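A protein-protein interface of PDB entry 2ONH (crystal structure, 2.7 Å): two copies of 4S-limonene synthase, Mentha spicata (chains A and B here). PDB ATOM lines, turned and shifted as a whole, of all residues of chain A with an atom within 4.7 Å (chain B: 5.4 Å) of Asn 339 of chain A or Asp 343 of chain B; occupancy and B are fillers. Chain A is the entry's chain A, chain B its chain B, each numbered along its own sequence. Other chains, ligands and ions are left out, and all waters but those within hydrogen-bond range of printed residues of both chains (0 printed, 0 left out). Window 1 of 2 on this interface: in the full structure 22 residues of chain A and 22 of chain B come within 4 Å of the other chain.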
ATOM      1  N   ASN A 248       3.211  -4.675  -9.484  1.00  0.00           N
ATOM      2  CA  ASN A 248       4.381  -5.458  -9.128  1.00  0.00           C
ATOM      3  C   ASN A 248       5.179  -5.892 -10.353  1.00  0.00           C
ATOM      4  O   ASN A 248       6.365  -5.648 -10.440  1.00  0.00           O
ATOM      5  CB  ASN A 248       3.977  -6.694  -8.334  1.00  0.00           C
ATOM      6  CG  ASN A 248       5.080  -7.174  -7.413  1.00  0.00           C
ATOM      7  OD1 ASN A 248       5.591  -8.305  -7.443  1.00  0.00           O
ATOM      8  ND2 ASN A 248       5.457  -6.238  -6.549  1.00  0.00           N
ATOM      9  N   LEU A 335       9.266 -15.199 -16.485  1.00  0.00           N
ATOM     10  CA  LEU A 335       9.364 -15.423 -15.063  1.00  0.00           C
ATOM     11  C   LEU A 335       8.023 -15.028 -14.442  1.00  0.00           C
ATOM     12  O   LEU A 335       7.477 -15.703 -13.586  1.00  0.00           O
ATOM     13  CB  LEU A 335      10.497 -14.585 -14.477  1.00  0.00           C
ATOM     14  CG  LEU A 335      10.880 -14.825 -13.013  1.00  0.00           C
ATOM     15  CD1 LEU A 335      11.199 -16.270 -12.747  1.00  0.00           C
ATOM     16  CD2 LEU A 335      12.191 -14.146 -12.726  1.00  0.00           C
ATOM     17  N   ALA A 336       7.490 -13.925 -14.898  1.00  0.00           N
ATOM     18  CA  ALA A 336       6.223 -13.455 -14.414  1.00  0.00           C
ATOM     19  C   ALA A 336       5.194 -14.552 -14.580  1.00  0.00           C
ATOM     20  O   ALA A 336       4.457 -14.892 -13.656  1.00  0.00           O
ATOM     21  CB  ALA A 336       5.727 -12.317 -15.235  1.00  0.00           C
ATOM     22  N   LEU A 337       5.148 -15.091 -15.779  1.00  0.00           N
ATOM     23  CA  LEU A 337       4.230 -16.161 -16.093  1.00  0.00           C
ATOM     24  C   LEU A 337       4.471 -17.286 -15.106  1.00  0.00           C
ATOM     25  O   LEU A 337       3.575 -17.688 -14.379  1.00  0.00           O
ATOM     26  CB  LEU A 337       4.477 -16.686 -17.504  1.00  0.00           C
ATOM     27  CG  LEU A 337       3.295 -16.908 -18.435  1.00  0.00           C
ATOM     28  CD1 LEU A 337       3.799 -17.273 -19.808  1.00  0.00           C
ATOM     29  CD2 LEU A 337       2.518 -18.138 -18.036  1.00  0.00           C
ATOM     30  N   ASN A 338       5.700 -17.784 -15.080  1.00  0.00           N
ATOM     31  CA  ASN A 338       6.038 -18.866 -14.190  1.00  0.00           C
ATOM     32  C   ASN A 338       5.567 -18.543 -12.792  1.00  0.00           C
ATOM     33  O   ASN A 338       5.018 -19.392 -12.120  1.00  0.00           O
ATOM     34  CB  ASN A 338       7.543 -19.127 -14.157  1.00  0.00           C
ATOM     35  CG  ASN A 338       7.919 -20.158 -13.120  1.00  0.00           C
ATOM     36  OD1 ASN A 338       7.940 -21.376 -13.269  1.00  0.00           O
ATOM     37  ND2 ASN A 338       8.224 -19.577 -11.973  1.00  0.00           N
ATOM     38  N   ASN A 339       5.779 -17.319 -12.372  1.00  0.00           N
ATOM     39  CA  ASN A 339       5.389 -16.907 -11.061  1.00  0.00           C
ATOM     40  C   ASN A 339       3.879 -16.968 -10.864  1.00  0.00           C
ATOM     41  O   ASN A 339       3.397 -17.332  -9.791  1.00  0.00           O
ATOM     42  CB  ASN A 339       5.884 -15.490 -10.808  1.00  0.00           C
ATOM     43  CG  ASN A 339       7.321 -15.451 -10.368  1.00  0.00           C
ATOM     44  OD1 ASN A 339       8.016 -16.452 -10.542  1.00  0.00           O
ATOM     45  ND2 ASN A 339       7.789 -14.334  -9.804  1.00  0.00           N
ATOM     46  N   PHE A 340       3.137 -16.607 -11.908  1.00  0.00           N
ATOM     47  CA  PHE A 340       1.683 -16.616 -11.851  1.00  0.00           C
ATOM     48  C   PHE A 340       1.041 -18.008 -11.829  1.00  0.00           C
ATOM     49  O   PHE A 340       0.199 -18.320 -10.962  1.00  0.00           O
ATOM     50  CB  PHE A 340       1.100 -15.853 -13.027  1.00  0.00           C
ATOM     51  CG  PHE A 340      -0.338 -16.125 -13.195  1.00  0.00           C
ATOM     52  CD1 PHE A 340      -1.192 -15.488 -12.327  1.00  0.00           C
ATOM     53  CD2 PHE A 340      -0.755 -17.032 -14.142  1.00  0.00           C
ATOM     54  CE1 PHE A 340      -2.526 -15.771 -12.400  1.00  0.00           C
ATOM     55  CE2 PHE A 340      -2.117 -17.306 -14.199  1.00  0.00           C
ATOM     56  CZ  PHE A 340      -2.991 -16.678 -13.333  1.00  0.00           C
ATOM     57  N   VAL A 341       1.397 -18.846 -12.795  1.00  0.00           N
ATOM     58  CA  VAL A 341       0.839 -20.110 -12.806  1.00  0.00           C
ATOM     59  C   VAL A 341       1.212 -20.799 -11.515  1.00  0.00           C
ATOM     60  O   VAL A 341       0.332 -21.378 -10.907  1.00  0.00           O
ATOM     61  CB  VAL A 341       1.293 -20.938 -13.990  1.00  0.00           C
ATOM     62  CG1 VAL A 341       2.088 -20.070 -14.906  1.00  0.00           C
ATOM     63  CG2 VAL A 341       2.049 -22.147 -13.531  1.00  0.00           C
ATOM     64  N   ASP A 342       2.507 -20.704 -11.087  1.00  0.00           N
ATOM     65  CA  ASP A 342       2.992 -21.353  -9.826  1.00  0.00           C
ATOM     66  C   ASP A 342       2.176 -20.894  -8.634  1.00  0.00           C
ATOM     67  O   ASP A 342       1.735 -21.745  -7.804  1.00  0.00           O
ATOM     68  CB  ASP A 342       4.462 -21.022  -9.569  1.00  0.00           C
ATOM     69  CG  ASP A 342       5.429 -22.005 -10.265  1.00  0.00           C
ATOM     70  OD1 ASP A 342       4.961 -22.930 -10.933  1.00  0.00           O
ATOM     71  OD2 ASP A 342       6.657 -21.824 -10.132  1.00  0.00           O
ATOM     72  N   ASP A 343       1.951 -19.545  -8.528  1.00  0.00           N
ATOM     73  CA  ASP A 343       1.158 -19.014  -7.396  1.00  0.00           C
ATOM     74  C   ASP A 343      -0.277 -19.493  -7.474  1.00  0.00           C
ATOM     75  O   ASP A 343      -0.897 -19.783  -6.442  1.00  0.00           O
ATOM     76  CB  ASP A 343       1.122 -17.487  -7.360  1.00  0.00           C
ATOM     77  CG  ASP A 343      -0.159 -16.944  -6.601  1.00  0.00           C
ATOM     78  OD1 ASP A 343      -0.412 -17.397  -5.463  1.00  0.00           O
ATOM     79  OD2 ASP A 343      -0.889 -16.091  -7.155  1.00  0.00           O
ATOM     80  N   LYS B 287       9.703 -13.622   5.872  1.00  0.00           N
ATOM     81  CA  LYS B 287       9.275 -14.876   5.256  1.00  0.00           C
ATOM     82  C   LYS B 287      10.315 -15.987   5.293  1.00  0.00           C
ATOM     83  O   LYS B 287      10.004 -17.147   5.598  1.00  0.00           O
ATOM     84  CB  LYS B 287       8.883 -14.641   3.803  1.00  0.00           C
ATOM     85  CG  LYS B 287       7.638 -13.819   3.590  1.00  0.00           C
ATOM     86  CD  LYS B 287       8.005 -12.816   2.504  1.00  0.00           C
ATOM     87  CE  LYS B 287       6.797 -12.278   1.730  1.00  0.00           C
ATOM     88  NZ  LYS B 287       7.159 -11.634   0.430  1.00  0.00           N
ATOM     89  N   ASN B 338       9.363 -22.846  -3.398  1.00  0.00           N
ATOM     90  CA  ASN B 338       9.595 -22.574  -4.796  1.00  0.00           C
ATOM     91  C   ASN B 338       9.007 -21.227  -5.137  1.00  0.00           C
ATOM     92  O   ASN B 338       9.650 -20.423  -5.793  1.00  0.00           O
ATOM     93  CB  ASN B 338       8.966 -23.643  -5.697  1.00  0.00           C
ATOM     94  CG  ASN B 338       8.845 -23.184  -7.164  1.00  0.00           C
ATOM     95  OD1 ASN B 338       7.847 -22.511  -7.399  1.00  0.00           O
ATOM     96  ND2 ASN B 338       9.740 -23.486  -8.106  1.00  0.00           N
ATOM     97  N   ASN B 339       7.805 -20.977  -4.692  1.00  0.00           N
ATOM     98  CA  ASN B 339       7.204 -19.735  -4.976  1.00  0.00           C
ATOM     99  C   ASN B 339       7.940 -18.599  -4.273  1.00  0.00           C
ATOM    100  O   ASN B 339       8.054 -17.486  -4.782  1.00  0.00           O
ATOM    101  CB  ASN B 339       5.740 -19.767  -4.563  1.00  0.00           C
ATOM    102  CG  ASN B 339       4.935 -20.722  -5.391  1.00  0.00           C
ATOM    103  OD1 ASN B 339       5.419 -21.393  -6.284  1.00  0.00           O
ATOM    104  ND2 ASN B 339       3.653 -20.775  -5.068  1.00  0.00           N
ATOM    105  N   PHE B 340       8.450 -18.875  -3.128  1.00  0.00           N
ATOM    106  CA  PHE B 340       9.152 -17.877  -2.429  1.00  0.00           C
ATOM    107  C   PHE B 340      10.390 -17.415  -3.184  1.00  0.00           C
ATOM    108  O   PHE B 340      10.505 -16.251  -3.546  1.00  0.00           O
ATOM    109  CB  PHE B 340       9.580 -18.359  -1.047  1.00  0.00           C
ATOM    110  CG  PHE B 340      10.528 -17.404  -0.405  1.00  0.00           C
ATOM    111  CD1 PHE B 340      10.040 -16.166  -0.069  1.00  0.00           C
ATOM    112  CD2 PHE B 340      11.857 -17.716  -0.251  1.00  0.00           C
ATOM    113  CE1 PHE B 340      10.893 -15.204   0.417  1.00  0.00           C
ATOM    114  CE2 PHE B 340      12.703 -16.724   0.246  1.00  0.00           C
ATOM    115  CZ  PHE B 340      12.229 -15.475   0.576  1.00  0.00           C
ATOM    116  N   VAL B 341      11.318 -18.319  -3.424  1.00  0.00           N
ATOM    117  CA  VAL B 341      12.502 -17.918  -4.101  1.00  0.00           C
ATOM    118  C   VAL B 341      12.201 -17.394  -5.485  1.00  0.00           C
ATOM    119  O   VAL B 341      12.804 -16.424  -5.913  1.00  0.00           O
ATOM    120  CB  VAL B 341      13.561 -19.061  -4.194  1.00  0.00           C
ATOM    121  CG1 VAL B 341      13.363 -19.997  -3.030  1.00  0.00           C
ATOM    122  CG2 VAL B 341      13.522 -19.726  -5.535  1.00  0.00           C
ATOM    123  N   ASP B 342      11.263 -18.021  -6.174  1.00  0.00           N
ATOM    124  CA  ASP B 342      10.911 -17.591  -7.505  1.00  0.00           C
ATOM    125  C   ASP B 342      10.436 -16.158  -7.433  1.00  0.00           C
ATOM    126  O   ASP B 342      10.840 -15.369  -8.260  1.00  0.00           O
ATOM    127  CB  ASP B 342       9.802 -18.460  -8.089  1.00  0.00           C
ATOM    128  CG  ASP B 342      10.329 -19.635  -8.887  1.00  0.00           C
ATOM    129  OD1 ASP B 342      11.543 -19.799  -8.953  1.00  0.00           O
ATOM    130  OD2 ASP B 342       9.510 -20.381  -9.436  1.00  0.00           O
ATOM    131  N   ASP B 343       9.572 -15.820  -6.434  1.00  0.00           N
ATOM    132  CA  ASP B 343       9.078 -14.425  -6.324  1.00  0.00           C
ATOM    133  C   ASP B 343      10.153 -13.468  -5.876  1.00  0.00           C
ATOM    134  O   ASP B 343      10.076 -12.288  -6.200  1.00  0.00           O
ATOM    135  CB  ASP B 343       7.927 -14.262  -5.338  1.00  0.00           C
ATOM    136  CG  ASP B 343       7.790 -12.768  -4.845  1.00  0.00           C
ATOM    137  OD1 ASP B 343       8.259 -12.446  -3.733  1.00  0.00           O
ATOM    138  OD2 ASP B 343       7.234 -11.943  -5.595  1.00  0.00           O
ATOM    139  N   THR B 344      11.117 -13.950  -5.118  1.00  0.00           N
ATOM    140  CA  THR B 344      12.151 -13.111  -4.686  1.00  0.00           C
ATOM    141  C   THR B 344      13.138 -12.811  -5.819  1.00  0.00           C
ATOM    142  O   THR B 344      13.501 -11.649  -6.028  1.00  0.00           O
ATOM    143  CB  THR B 344      12.838 -13.699  -3.576  1.00  0.00           C
ATOM    144  OG1 THR B 344      11.932 -13.817  -2.471  1.00  0.00           O
ATOM    145  CG2 THR B 344      13.981 -12.791  -3.188  1.00  0.00           C
ATOM    146  N   SER B 345      13.559 -13.835  -6.573  1.00  0.00           N
ATOM    147  CA  SER B 345      14.496 -13.591  -7.664  1.00  0.00           C
ATOM    148  C   SER B 345      13.912 -12.615  -8.679  1.00  0.00           C
ATOM    149  O   SER B 345      14.657 -11.873  -9.337  1.00  0.00           O
ATOM    150  CB  SER B 345      14.870 -14.895  -8.357  1.00  0.00           C
ATOM    151  OG  SER B 345      14.785 -15.935  -7.409  1.00  0.00           O
ATOM    152  N   TYR B 346      12.574 -12.621  -8.806  1.00  0.00           N
ATOM    153  CA  TYR B 346      11.893 -11.721  -9.723  1.00  0.00           C
ATOM    154  C   TYR B 346      12.203 -10.289  -9.298  1.00  0.00           C
ATOM    155  O   TYR B 346      12.822  -9.542 -10.043  1.00  0.00           O
ATOM    156  CB  TYR B 346      10.368 -11.953  -9.703  1.00  0.00           C
ATOM    157  CG  TYR B 346       9.627 -11.091 -10.754  1.00  0.00           C
ATOM    158  CD1 TYR B 346       9.654 -11.483 -12.085  1.00  0.00           C
ATOM    159  CD2 TYR B 346       8.982  -9.904 -10.428  1.00  0.00           C
ATOM    160  CE1 TYR B 346       9.070 -10.705 -13.087  1.00  0.00           C
ATOM    161  CE2 TYR B 346       8.389  -9.112 -11.417  1.00  0.00           C
ATOM    162  CZ  TYR B 346       8.443  -9.511 -12.753  1.00  0.00           C
ATOM    163  OH  TYR B 346       7.970  -8.760 -13.720  1.00  0.00           O
ATOM    164  N   ASP B 347      11.774  -9.920  -8.084  1.00  0.00           N
ATOM    165  CA  ASP B 347      12.014  -8.594  -7.572  1.00  0.00           C
ATOM    166  C   ASP B 347      13.465  -8.225  -7.777  1.00  0.00           C
ATOM    167  O   ASP B 347      13.759  -7.117  -8.190  1.00  0.00           O
ATOM    168  CB  ASP B 347      11.683  -8.523  -6.090  1.00  0.00           C
ATOM    169  CG  ASP B 347      10.220  -8.489  -5.835  1.00  0.00           C
ATOM    170  OD1 ASP B 347       9.840  -8.443  -4.678  1.00  0.00           O
ATOM    171  OD2 ASP B 347       9.459  -8.507  -6.788  1.00  0.00           O
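Of the 11 printed residues of chain B, 6 touch a printed residue of chain A. Hydrophobic or aromatic side chains of chain B that line the printed part of chain A: Tyr 346. Among the printed residues, 10 pairs touch across the chains. Among the printed residues, no Asp or Glu carboxylate lies within 4 Å of a Lys or Arg side-chain nitrogen of the other chain.
Of the printed residues of chain B, Leu 335 of chain A touches Tyr 346 (3.7 Å). Leu 337 of chain A touches none of the printed residues of chain B. Of chain B, only Asp 342, Asp 343 and Tyr 346 come within 4 Å of Asn 339 of chain A. Val 341 of chain A touches none of the printed residues of chain B. Of the printed residues of chain A, Asn 339 of chain B touches Asp 342 (3.4 Å) and Asp 343 (3.8 Å). Of the printed residues of chain A, Asp 342 of chain B touches Asn 338 (3.0 Å), Asn 339 (3.6 Å) and Asp 342 (3.3 Å). Of chain A, only Asn 339 comes within 4 Å of Asp 343 of chain B. Printed residues of chain A within 4 Å of Tyr 346 of chain B: Leu 335 and Asn 339. The nearest printed residue of chain B that does not touch Asn 339 of chain A is Asn 339 of chain B (5.7 Å). The nearest residue of chain A that does not touch Asp 343 of chain B is Asn 248 of chain A (4.4 Å).
O of Leu 335 of chain A lies close to OD1 of Asn 339 of chain A (3.2 Å). The side-chain amide nitrogen (ND2) of Asn 338 of chain A sits at hydrogen-bond distance from the side-chain amide oxygen (OD1) of Asn 339 of chain A (3.4 Å). The side-chain carboxylate (OD2) of Asp 342 of chain A sits at hydrogen-bond distance from the side-chain amide nitrogen (ND2) of Asn 338 of chain A, 3.3 Å away. The side-chain amide oxygen of Asn 339 of chain B lies close to the side-chain amide oxygen of Asn 338 of chain B, at 2.9 Å. The side-chain carboxylate of Asp 342 of chain B lies close to the side-chain amide oxygen of Asn 338 of chain B (3.4 Å).
Asn 338 of chain A touches Asp 342 of chain B, and with the chains exchanged Asp 342 of chain A touches Asn 338 of chain B. Asn 339 of chain A touches Asp 342 of chain B, and with the chains exchanged Asp 342 of chain A touches Asn 339 of chain B. Asn 339 of chain A touches Asp 343 of chain B, and with the chains exchanged Asp 343 of chain A touches Asn 339 of chain B. Asp 342 of chain B touches its own counterpart, Asp 342 of chain A. Positions printed for both chains: 338, 339, 340, 341, 342 and 343. Of the 10 pairs that touch across the chains among the printed residues, 7 have their exchanged pair printed and touching as well.
Among the printed residues, pairs that only touch across the chains: Asn 248 of chain A with Asp 347 of chain B, Leu 335 of chain A with Tyr 346 of chain B, Asn 339 of chain A with Asp 342 of chain B, Asn 339 of chain A with Asp 343 of chain B, Asn 339 of chain A with Tyr 346 of chain B and Asp 343 of chain A with Asn 339 of chain B.
OD2 of Asp 342 of chain B is in hydrogen-bond range of ND2 of Asn 338 of chain A (3.0 Å). The side-chain carboxylate of Asp 342 of chain A lies close to the side-chain amide oxygen of Asn 338 of chain B (3.1 Å). The backbone carbonyl oxygen of Asp 342 of chain A lies within hydrogen-bond range of the side-chain amide nitrogen of Asn 339 of chain B (3.5 Å). OD2 of Asp 342 of chain A lies close to OD2 of Asp 342 of chain B (3.3 Å).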
